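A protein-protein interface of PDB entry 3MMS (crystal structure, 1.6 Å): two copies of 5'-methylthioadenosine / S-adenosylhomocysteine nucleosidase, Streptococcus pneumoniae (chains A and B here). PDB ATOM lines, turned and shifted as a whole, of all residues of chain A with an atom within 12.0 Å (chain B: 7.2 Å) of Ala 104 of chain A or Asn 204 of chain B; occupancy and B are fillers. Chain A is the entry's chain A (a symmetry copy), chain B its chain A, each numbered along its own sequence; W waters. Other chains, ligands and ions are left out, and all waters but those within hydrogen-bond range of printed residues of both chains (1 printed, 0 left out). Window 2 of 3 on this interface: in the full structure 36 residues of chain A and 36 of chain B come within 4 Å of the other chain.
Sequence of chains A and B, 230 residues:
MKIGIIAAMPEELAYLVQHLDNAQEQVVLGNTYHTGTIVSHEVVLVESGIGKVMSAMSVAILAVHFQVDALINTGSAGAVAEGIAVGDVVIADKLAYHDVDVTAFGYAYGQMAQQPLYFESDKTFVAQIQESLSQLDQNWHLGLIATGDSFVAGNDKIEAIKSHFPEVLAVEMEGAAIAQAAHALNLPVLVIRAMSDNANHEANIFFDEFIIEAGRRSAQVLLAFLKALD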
ATOM      1  N   ASP A  99      15.706  25.895  20.705  1.00  0.00           N
ATOM      2  CA  ASP A  99      15.255  24.730  19.942  1.00  0.00           C
ATOM      3  C   ASP A  99      14.241  23.830  20.640  1.00  0.00           C
ATOM      4  O   ASP A  99      14.049  22.674  20.245  1.00  0.00           O
ATOM      5  CB  ASP A  99      16.482  23.886  19.530  1.00  0.00           C
ATOM      6  CG  ASP A  99      17.210  23.229  20.719  1.00  0.00           C
ATOM      7  OD1 ASP A  99      16.917  23.533  21.895  1.00  0.00           O
ATOM      8  OD2 ASP A  99      18.107  22.379  20.454  1.00  0.00           O
ATOM      9  N   VAL A 100      13.570  24.378  21.652  1.00  0.00           N
ATOM     10  CA  VAL A 100      12.597  23.634  22.445  1.00  0.00           C
ATOM     11  C   VAL A 100      11.181  24.076  22.138  1.00  0.00           C
ATOM     12  O   VAL A 100      10.884  25.269  22.164  1.00  0.00           O
ATOM     13  CB  VAL A 100      12.886  23.870  23.979  1.00  0.00           C
ATOM     14  CG1 VAL A 100      11.719  23.371  24.856  1.00  0.00           C
ATOM     15  CG2 VAL A 100      14.188  23.138  24.370  1.00  0.00           C
ATOM     16  N   ASP A 101      10.320  23.107  21.846  1.00  0.00           N
ATOM     17  CA  ASP A 101       8.915  23.390  21.567  1.00  0.00           C
ATOM     18  C   ASP A 101       7.994  22.422  22.297  1.00  0.00           C
ATOM     19  O   ASP A 101       7.810  21.260  21.894  1.00  0.00           O
ATOM     20  CB  ASP A 101       8.629  23.356  20.053  1.00  0.00           C
ATOM     21  CG  ASP A 101       7.194  23.788  19.698  1.00  0.00           C
ATOM     22  OD1 ASP A 101       6.280  23.736  20.562  1.00  0.00           O
ATOM     23  OD2 ASP A 101       6.968  24.165  18.522  1.00  0.00           O
ATOM     24  N   VAL A 102       7.440  22.897  23.419  1.00  0.00           N
ATOM     25  CA  VAL A 102       6.448  22.117  24.155  1.00  0.00           C
ATOM     26  C   VAL A 102       5.217  23.039  24.211  1.00  0.00           C
ATOM     27  O   VAL A 102       4.413  23.010  25.159  1.00  0.00           O
ATOM     28  CB  VAL A 102       6.914  21.764  25.585  1.00  0.00           C
ATOM     29  CG1 VAL A 102       5.989  20.712  26.198  1.00  0.00           C
ATOM     30  CG2 VAL A 102       8.331  21.226  25.535  1.00  0.00           C
ATOM     31  N   THR A 103       5.062  23.839  23.161  1.00  0.00           N
ATOM     32  CA  THR A 103       3.946  24.787  23.122  1.00  0.00           C
ATOM     33  C   THR A 103       2.574  24.113  23.072  1.00  0.00           C
ATOM     34  O   THR A 103       1.560  24.743  23.400  1.00  0.00           O
ATOM     35  CB  THR A 103       4.074  25.785  21.930  1.00  0.00           C
ATOM     36  OG1 THR A 103       4.024  25.082  20.684  1.00  0.00           O
ATOM     37  CG2 THR A 103       5.386  26.577  22.041  1.00  0.00           C
ATOM     38  N   ALA A 104       2.527  22.842  22.686  1.00  0.00           N
ATOM     39  CA  ALA A 104       1.254  22.123  22.642  1.00  0.00           C
ATOM     40  C   ALA A 104       0.576  22.108  24.014  1.00  0.00           C
ATOM     41  O   ALA A 104      -0.656  21.985  24.096  1.00  0.00           O
ATOM     42  CB  ALA A 104       1.477  20.699  22.165  1.00  0.00           C
ATOM     43  N   PHE A 105       1.362  22.231  25.086  1.00  0.00           N
ATOM     44  CA  PHE A 105       0.798  22.231  26.443  1.00  0.00           C
ATOM     45  C   PHE A 105       0.710  23.617  27.058  1.00  0.00           C
ATOM     46  O   PHE A 105       0.450  23.742  28.249  1.00  0.00           O
ATOM     47  CB  PHE A 105       1.601  21.298  27.356  1.00  0.00           C
ATOM     48  CG  PHE A 105       1.391  19.836  27.037  1.00  0.00           C
ATOM     49  CD1 PHE A 105       0.301  19.144  27.566  1.00  0.00           C
ATOM     50  CD2 PHE A 105       2.259  19.157  26.193  1.00  0.00           C
ATOM     51  CE1 PHE A 105       0.087  17.809  27.262  1.00  0.00           C
ATOM     52  CE2 PHE A 105       2.041  17.814  25.891  1.00  0.00           C
ATOM     53  CZ  PHE A 105       0.962  17.144  26.424  1.00  0.00           C
ATOM     54  N   GLY A 106       0.965  24.640  26.243  1.00  0.00           N
ATOM     55  CA  GLY A 106       0.855  26.019  26.701  1.00  0.00           C
ATOM     56  C   GLY A 106       2.140  26.707  27.110  1.00  0.00           C
ATOM     57  O   GLY A 106       2.135  27.902  27.438  1.00  0.00           O
ATOM     58  N   TYR A 107       3.239  25.964  27.149  1.00  0.00           N
ATOM     59  CA  TYR A 107       4.522  26.570  27.507  1.00  0.00           C
ATOM     60  C   TYR A 107       4.930  27.600  26.443  1.00  0.00           C
ATOM     61  O   TYR A 107       4.490  27.524  25.278  1.00  0.00           O
ATOM     62  CB  TYR A 107       5.602  25.493  27.568  1.00  0.00           C
ATOM     63  CG  TYR A 107       5.443  24.550  28.727  1.00  0.00           C
ATOM     64  CD1 TYR A 107       5.792  24.947  30.027  1.00  0.00           C
ATOM     65  CD2 TYR A 107       4.961  23.254  28.536  1.00  0.00           C
ATOM     66  CE1 TYR A 107       5.672  24.082  31.085  1.00  0.00           C
ATOM     67  CE2 TYR A 107       4.827  22.383  29.605  1.00  0.00           C
ATOM     68  CZ  TYR A 107       5.191  22.809  30.870  1.00  0.00           C
ATOM     69  OH  TYR A 107       5.093  21.943  31.924  1.00  0.00           O
ATOM     70  N   ALA A 108       5.770  28.559  26.830  1.00  0.00           N
ATOM     71  CA  ALA A 108       6.264  29.544  25.873  1.00  0.00           C
ATOM     72  C   ALA A 108       7.246  28.819  24.948  1.00  0.00           C
ATOM     73  O   ALA A 108       7.858  27.822  25.348  1.00  0.00           O
ATOM     74  CB  ALA A 108       7.015  30.664  26.608  1.00  0.00           C
ATOM     75  N   TYR A 109       7.396  29.300  23.722  1.00  0.00           N
ATOM     76  CA  TYR A 109       8.367  28.660  22.840  1.00  0.00           C
ATOM     77  C   TYR A 109       9.744  28.760  23.521  1.00  0.00           C
ATOM     78  O   TYR A 109      10.094  29.810  24.067  1.00  0.00           O
ATOM     79  CB  TYR A 109       8.427  29.363  21.477  1.00  0.00           C
ATOM     80  CG  TYR A 109       9.408  28.668  20.565  1.00  0.00           C
ATOM     81  CD1 TYR A 109      10.757  28.998  20.618  1.00  0.00           C
ATOM     82  CD2 TYR A 109       9.007  27.602  19.746  1.00  0.00           C
ATOM     83  CE1 TYR A 109      11.700  28.287  19.892  1.00  0.00           C
ATOM     84  CE2 TYR A 109       9.959  26.873  18.997  1.00  0.00           C
ATOM     85  CZ  TYR A 109      11.307  27.242  19.098  1.00  0.00           C
ATOM     86  OH  TYR A 109      12.296  26.566  18.415  1.00  0.00           O
ATOM     87  N   GLY A 110      10.503  27.661  23.514  1.00  0.00           N
ATOM     88  CA  GLY A 110      11.819  27.670  24.128  1.00  0.00           C
ATOM     89  C   GLY A 110      11.806  27.147  25.554  1.00  0.00           C
ATOM     90  O   GLY A 110      12.853  26.772  26.081  1.00  0.00           O
ATOM     91  N   GLN A 111      10.626  27.123  26.175  1.00  0.00           N
ATOM     92  CA  GLN A 111      10.506  26.677  27.551  1.00  0.00           C
ATOM     93  C   GLN A 111      10.363  25.167  27.670  1.00  0.00           C
ATOM     94  O   GLN A 111       9.408  24.583  27.151  1.00  0.00           O
ATOM     95  CB  GLN A 111       9.302  27.374  28.196  1.00  0.00           C
ATOM     96  CG  GLN A 111       9.075  27.012  29.673  1.00  0.00           C
ATOM     97  CD  GLN A 111       7.838  27.714  30.237  1.00  0.00           C
ATOM     98  OE1 GLN A 111       7.065  28.334  29.497  1.00  0.00           O
ATOM     99  NE2 GLN A 111       7.645  27.616  31.542  1.00  0.00           N
ATOM    100  N   MET A 112      11.324  24.529  28.339  1.00  0.00           N
ATOM    101  CA  MET A 112      11.210  23.087  28.547  1.00  0.00           C
ATOM    102  C   MET A 112      10.103  22.808  29.574  1.00  0.00           C
ATOM    103  O   MET A 112       9.841  23.616  30.485  1.00  0.00           O
ATOM    104  CB  MET A 112      12.566  22.537  29.029  1.00  0.00           C
ATOM    105  CG  MET A 112      12.601  21.070  29.456  1.00  0.00           C
ATOM    106  SD  MET A 112      11.942  19.903  28.219  1.00  0.00           S
ATOM    107  CE  MET A 112      12.970  20.268  26.762  1.00  0.00           C
ATOM    108  N   ALA A 113       9.410  21.688  29.408  1.00  0.00           N
ATOM    109  CA  ALA A 113       8.353  21.311  30.344  1.00  0.00           C
ATOM    110  C   ALA A 113       8.902  21.268  31.766  1.00  0.00           C
ATOM    111  O   ALA A 113      10.032  20.800  31.996  1.00  0.00           O
ATOM    112  CB  ALA A 113       7.776  19.925  29.962  1.00  0.00           C
ATOM    113  N   GLN A 114       8.105  21.738  32.721  1.00  0.00           N
ATOM    114  CA  GLN A 114       8.449  21.766  34.138  1.00  0.00           C
ATOM    115  C   GLN A 114       9.743  22.563  34.415  1.00  0.00           C
ATOM    116  O   GLN A 114      10.477  22.294  35.363  1.00  0.00           O
ATOM    117  CB  GLN A 114       8.562  20.311  34.654  1.00  0.00           C
ATOM    118  CG  GLN A 114       7.269  19.510  34.274  1.00  0.00           C
ATOM    119  CD  GLN A 114       7.192  18.072  34.793  1.00  0.00           C
ATOM    120  OE1 GLN A 114       8.194  17.341  34.863  1.00  0.00           O
ATOM    121  NE2 GLN A 114       5.974  17.648  35.133  1.00  0.00           N
ATOM    122  N   HIS A 164      12.293  34.388  17.839  1.00  0.00           N
ATOM    123  CA  HIS A 164      11.786  33.926  19.125  1.00  0.00           C
ATOM    124  C   HIS A 164      12.379  34.756  20.259  1.00  0.00           C
ATOM    125  O   HIS A 164      11.700  35.057  21.241  1.00  0.00           O
ATOM    126  CB  HIS A 164      12.165  32.457  19.372  1.00  0.00           C
ATOM    127  CG  HIS A 164      11.541  31.486  18.415  1.00  0.00           C
ATOM    128  ND1 HIS A 164      10.178  31.270  18.353  1.00  0.00           N
ATOM    129  CD2 HIS A 164      12.098  30.624  17.533  1.00  0.00           C
ATOM    130  CE1 HIS A 164       9.925  30.314  17.477  1.00  0.00           C
ATOM    131  NE2 HIS A 164      11.071  29.905  16.966  1.00  0.00           N
ATOM    132  N   PHE B 151       7.755  18.420  22.128  1.00  0.00           N
ATOM    133  CA  PHE B 151       6.617  17.520  22.131  1.00  0.00           C
ATOM    134  C   PHE B 151       6.038  17.699  20.740  1.00  0.00           C
ATOM    135  O   PHE B 151       5.651  18.801  20.363  1.00  0.00           O
ATOM    136  CB  PHE B 151       5.594  17.930  23.195  1.00  0.00           C
ATOM    137  CG  PHE B 151       4.437  16.988  23.281  1.00  0.00           C
ATOM    138  CD1 PHE B 151       4.506  15.847  24.083  1.00  0.00           C
ATOM    139  CD2 PHE B 151       3.295  17.213  22.522  1.00  0.00           C
ATOM    140  CE1 PHE B 151       3.433  14.938  24.114  1.00  0.00           C
ATOM    141  CE2 PHE B 151       2.233  16.311  22.551  1.00  0.00           C
ATOM    142  CZ  PHE B 151       2.309  15.177  23.349  1.00  0.00           C
ATOM    143  N   VAL B 152       6.000  16.617  19.966  1.00  0.00           N
ATOM    144  CA  VAL B 152       5.526  16.647  18.573  1.00  0.00           C
ATOM    145  C   VAL B 152       4.006  16.620  18.526  1.00  0.00           C
ATOM    146  O   VAL B 152       3.380  15.688  19.019  1.00  0.00           O
ATOM    147  CB  VAL B 152       6.132  15.448  17.788  1.00  0.00           C
ATOM    148  CG1 VAL B 152       5.743  15.519  16.300  1.00  0.00           C
ATOM    149  CG2 VAL B 152       7.666  15.462  17.919  1.00  0.00           C
ATOM    150  N   ALA B 153       3.420  17.650  17.921  1.00  0.00           N
ATOM    151  CA  ALA B 153       1.957  17.760  17.882  1.00  0.00           C
ATOM    152  C   ALA B 153       1.517  18.426  16.599  1.00  0.00           C
ATOM    153  O   ALA B 153       0.932  19.518  16.611  1.00  0.00           O
ATOM    154  CB  ALA B 153       1.471  18.561  19.079  1.00  0.00           C
ATOM    155  N   ASP B 197      -0.354   8.513  21.823  1.00  0.00           N
ATOM    156  CA  ASP B 197      -0.944   9.447  20.882  1.00  0.00           C
ATOM    157  C   ASP B 197      -0.276   9.278  19.518  1.00  0.00           C
ATOM    158  O   ASP B 197       0.608   8.419  19.359  1.00  0.00           O
ATOM    159  CB  ASP B 197      -0.757  10.902  21.403  1.00  0.00           C
ATOM    160  CG  ASP B 197       0.708  11.273  21.609  1.00  0.00           C
ATOM    161  OD1 ASP B 197       1.345  11.726  20.635  1.00  0.00           O
ATOM    162  OD2 ASP B 197       1.211  11.092  22.741  1.00  0.00           O
ATOM    163  N   ALA B 199       1.095  11.982  17.840  1.00  0.00           N
ATOM    164  CA  ALA B 199       1.999  13.105  17.624  1.00  0.00           C
ATOM    165  C   ALA B 199       1.445  14.094  16.605  1.00  0.00           C
ATOM    166  O   ALA B 199       2.198  14.826  15.972  1.00  0.00           O
ATOM    167  CB  ALA B 199       3.361  12.601  17.179  1.00  0.00           C
ATOM    168  N   ASN B 200       0.125  14.113  16.459  1.00  0.00           N
ATOM    169  CA  ASN B 200      -0.534  15.014  15.520  1.00  0.00           C
ATOM    170  C   ASN B 200      -1.107  16.248  16.214  1.00  0.00           C
ATOM    171  O   ASN B 200      -0.742  16.561  17.339  1.00  0.00           O
ATOM    172  CB  ASN B 200      -1.637  14.278  14.766  1.00  0.00           C
ATOM    173  CG  ASN B 200      -2.670  13.689  15.695  1.00  0.00           C
ATOM    174  OD1 ASN B 200      -2.754  14.073  16.854  1.00  0.00           O
ATOM    175  ND2 ASN B 200      -3.455  12.748  15.192  1.00  0.00           N
ATOM    176  N   HIS B 201      -2.003  16.950  15.531  1.00  0.00           N
ATOM    177  CA  HIS B 201      -2.553  18.190  16.067  1.00  0.00           C
ATOM    178  C   HIS B 201      -3.320  17.994  17.375  1.00  0.00           C
ATOM    179  O   HIS B 201      -3.544  18.946  18.114  1.00  0.00           O
ATOM    180  CB  HIS B 201      -3.447  18.875  15.030  1.00  0.00           C
ATOM    181  N   GLU B 202      -3.717  16.761  17.659  1.00  0.00           N
ATOM    182  CA  GLU B 202      -4.484  16.471  18.865  1.00  0.00           C
ATOM    183  C   GLU B 202      -3.635  15.781  19.926  1.00  0.00           C
ATOM    184  O   GLU B 202      -4.159  15.264  20.910  1.00  0.00           O
ATOM    185  CB  GLU B 202      -5.707  15.613  18.535  1.00  0.00           C
ATOM    186  CG  GLU B 202      -6.603  16.195  17.453  1.00  0.00           C
ATOM    187  CD  GLU B 202      -7.173  17.547  17.830  1.00  0.00           C
ATOM    188  OE1 GLU B 202      -7.320  17.816  19.040  1.00  0.00           O
ATOM    189  OE2 GLU B 202      -7.473  18.341  16.916  1.00  0.00           O
ATOM    190  N   ALA B 203      -2.323  15.776  19.718  1.00  0.00           N
ATOM    191  CA  ALA B 203      -1.436  14.888  20.458  1.00  0.00           C
ATOM    192  C   ALA B 203      -1.511  15.141  21.960  1.00  0.00           C
ATOM    193  O   ALA B 203      -1.520  14.203  22.755  1.00  0.00           O
ATOM    194  CB  ALA B 203      -0.006  15.032  19.964  1.00  0.00           C
ATOM    195  N   ASN B 204      -1.559  16.411  22.345  1.00  0.00           N
ATOM    196  CA  ASN B 204      -1.609  16.764  23.757  1.00  0.00           C
ATOM    197  C   ASN B 204      -2.888  16.269  24.420  1.00  0.00           C
ATOM    198  O   ASN B 204      -2.884  15.892  25.590  1.00  0.00           O
ATOM    199  CB  ASN B 204      -1.452  18.274  23.953  1.00  0.00           C
ATOM    200  CG  ASN B 204      -2.526  19.072  23.242  1.00  0.00           C
ATOM    201  OD1 ASN B 204      -3.407  19.651  23.876  1.00  0.00           O
ATOM    202  ND2 ASN B 204      -2.454  19.111  21.919  1.00  0.00           N
ATOM    203  N   ILE B 205      -3.979  16.264  23.661  1.00  0.00           N
ATOM    204  CA  ILE B 205      -5.264  15.795  24.180  1.00  0.00           C
ATOM    205  C   ILE B 205      -5.247  14.288  24.445  1.00  0.00           C
ATOM    206  O   ILE B 205      -5.675  13.807  25.506  1.00  0.00           O
ATOM    207  CB  ILE B 205      -6.386  16.116  23.167  1.00  0.00           C
ATOM    208  CG1 ILE B 205      -6.523  17.634  23.024  1.00  0.00           C
ATOM    209  CG2 ILE B 205      -7.699  15.450  23.600  1.00  0.00           C
ATOM    210  CD1 ILE B 205      -6.938  18.358  24.295  1.00  0.00           C
ATOM    211  N   PHE B 206      -4.739  13.527  23.482  1.00  0.00           N
ATOM    212  CA  PHE B 206      -4.724  12.091  23.653  1.00  0.00           C
ATOM    213  C   PHE B 206      -3.631  11.649  24.629  1.00  0.00           C
ATOM    214  O   PHE B 206      -3.800  10.670  25.339  1.00  0.00           O
ATOM    215  CB  PHE B 206      -4.649  11.404  22.281  1.00  0.00           C
ATOM    216  CG  PHE B 206      -5.943  11.503  21.539  1.00  0.00           C
ATOM    217  CD1 PHE B 206      -6.962  10.590  21.779  1.00  0.00           C
ATOM    218  CD2 PHE B 206      -6.204  12.591  20.720  1.00  0.00           C
ATOM    219  CE1 PHE B 206      -8.227  10.761  21.224  1.00  0.00           C
ATOM    220  CE2 PHE B 206      -7.476  12.776  20.159  1.00  0.00           C
ATOM    221  CZ  PHE B 206      -8.480  11.860  20.416  1.00  0.00           C
ATOM    222  N   PHE B 207      -2.521  12.386  24.674  1.00  0.00           N
ATOM    223  CA  PHE B 207      -1.478  12.116  25.656  1.00  0.00           C
ATOM    224  C   PHE B 207      -2.139  12.221  27.062  1.00  0.00           C
ATOM    225  O   PHE B 207      -1.986  11.320  27.904  1.00  0.00           O
ATOM    226  CB  PHE B 207      -0.367  13.165  25.540  1.00  0.00           C
ATOM    227  CG  PHE B 207       0.623  13.115  26.664  1.00  0.00           C
ATOM    228  CD1 PHE B 207       0.396  13.831  27.844  1.00  0.00           C
ATOM    229  CD2 PHE B 207       1.767  12.321  26.560  1.00  0.00           C
ATOM    230  CE1 PHE B 207       1.294  13.757  28.910  1.00  0.00           C
ATOM    231  CE2 PHE B 207       2.678  12.237  27.614  1.00  0.00           C
ATOM    232  CZ  PHE B 207       2.448  12.954  28.795  1.00  0.00           C
ATOM    233  N   ASP B 208      -2.884  13.303  27.305  1.00  0.00           N
ATOM    234  CA  ASP B 208      -3.509  13.471  28.632  1.00  0.00           C
ATOM    235  C   ASP B 208      -4.464  12.314  28.963  1.00  0.00           C
ATOM    236  O   ASP B 208      -4.526  11.843  30.102  1.00  0.00           O
ATOM    237  CB  ASP B 208      -4.283  14.803  28.725  1.00  0.00           C
ATOM    238  CG  ASP B 208      -3.381  16.015  28.891  1.00  0.00           C
ATOM    239  OD1 ASP B 208      -2.217  15.867  29.344  1.00  0.00           O
ATOM    240  OD2 ASP B 208      -3.860  17.143  28.595  1.00  0.00           O
ATOM    241  N   GLU B 209      -5.204  11.837  27.976  1.00  0.00           N
ATOM    242  CA  GLU B 209      -6.135  10.756  28.255  1.00  0.00           C
ATOM    243  C   GLU B 209      -5.514   9.401  28.477  1.00  0.00           C
ATOM    244  O   GLU B 209      -5.968   8.633  29.337  1.00  0.00           O
ATOM    245  CB  GLU B 209      -7.145  10.613  27.119  1.00  0.00           C
ATOM    246  CG  GLU B 209      -8.009  11.850  26.907  1.00  0.00           C
ATOM    247  CD  GLU B 209      -8.727  12.290  28.172  1.00  0.00           C
ATOM    248  OE1 GLU B 209      -9.338  11.436  28.840  1.00  0.00           O
ATOM    249  OE2 GLU B 209      -8.682  13.491  28.473  1.00  0.00           O
HETATM  250  O   HOH W   1       4.699  21.349  21.142  1.00  0.00           O
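Water W1 lies within hydrogen-bond range of O of Phe 151 of chain B (2.8 Å), OD1 of Asp 101 of chain A (2.9 Å), N of Ala 104 of chain A (3.1 Å) and N of Thr 103 of chain A (3.2 Å).
Printed residues of chain B within 4 Å of Asp 101 of chain A: Phe 151.
Of the printed residues of chain B, Phe 105 of chain A touches Phe 151 (3.6 Å), Asn 204 (3.6 Å), Phe 207 (3.6 Å) and Asp 208 (3.7 Å).
Of chain A, only Asp 101 (2.9 Å), Ala 104 (3.9 Å) and Phe 105 (3.6 Å) come within 4 Å of Phe 151 of chain B.
No residue of chain A comes within 4 Å of Glu 202 of chain B.
No residue of chain A comes within 4 Å of Ala 203 of chain B.
Asn 204 of chain B touches just these residues of chain A: Ala 104 (3.6 Å) and Phe 105 (3.6 Å).
No residue of chain A comes within 4 Å of Ile 205 of chain B.
Phe 207 of chain B touches one residue of chain A.
Asp 208 of chain B touches just one residue of chain A: Phe 105 (3.7 Å).
The nearest residue of chain A that does not touch Asn 204 of chain B is Thr 103 of chain A (7.0 Å).
The nearest printed residue of chain B that does not touch Asp 101 of chain A is Val 152 of chain B (5.3 Å).
N of Phe 151 of chain B sits at hydrogen-bond distance from O of Asp 101 of chain A (2.9 Å).
The side-chain hydroxyl of Thr 103 of chain A lies within hydrogen-bond range of the side-chain carboxylate of Asp 101 of chain A (2.6 Å).
No position is printed for both chains.
Of the 8 pairs that touch across the chains among the printed residues, none has its exchanged pair printed and touching as well.
CD2 of Phe 151 of chain B touches CB of Ala 104 of chain A (3.9 Å).
Ala 104 of chain A touches Ala 153 of chain B.
Asn 204 of chain B touches Ala 104 of chain A.
Phe 105 of chain A touches Phe 151 of chain B.
Phe 105 of chain A touches Asn 204 of chain B (CZ to CB, 3.6 Å).
CZ of Phe 105 of chain A touches CD1 of Phe 207 of chain B, at 3.6 Å.
CE1 of Phe 105 of chain A touches OD1 of Asp 208 of chain B, at 3.7 Å.
Hydrophobic or aromatic side chains of chain A that line the printed part of chain B: Ala 104 and Phe 105.
Along chain A the printed residues that touch a printed residue of chain B span positions 101 to 105.
Hydrophobic or aromatic side chains of chain B that line the printed part of chain A: Phe 151, Ala 153 and Phe 207.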
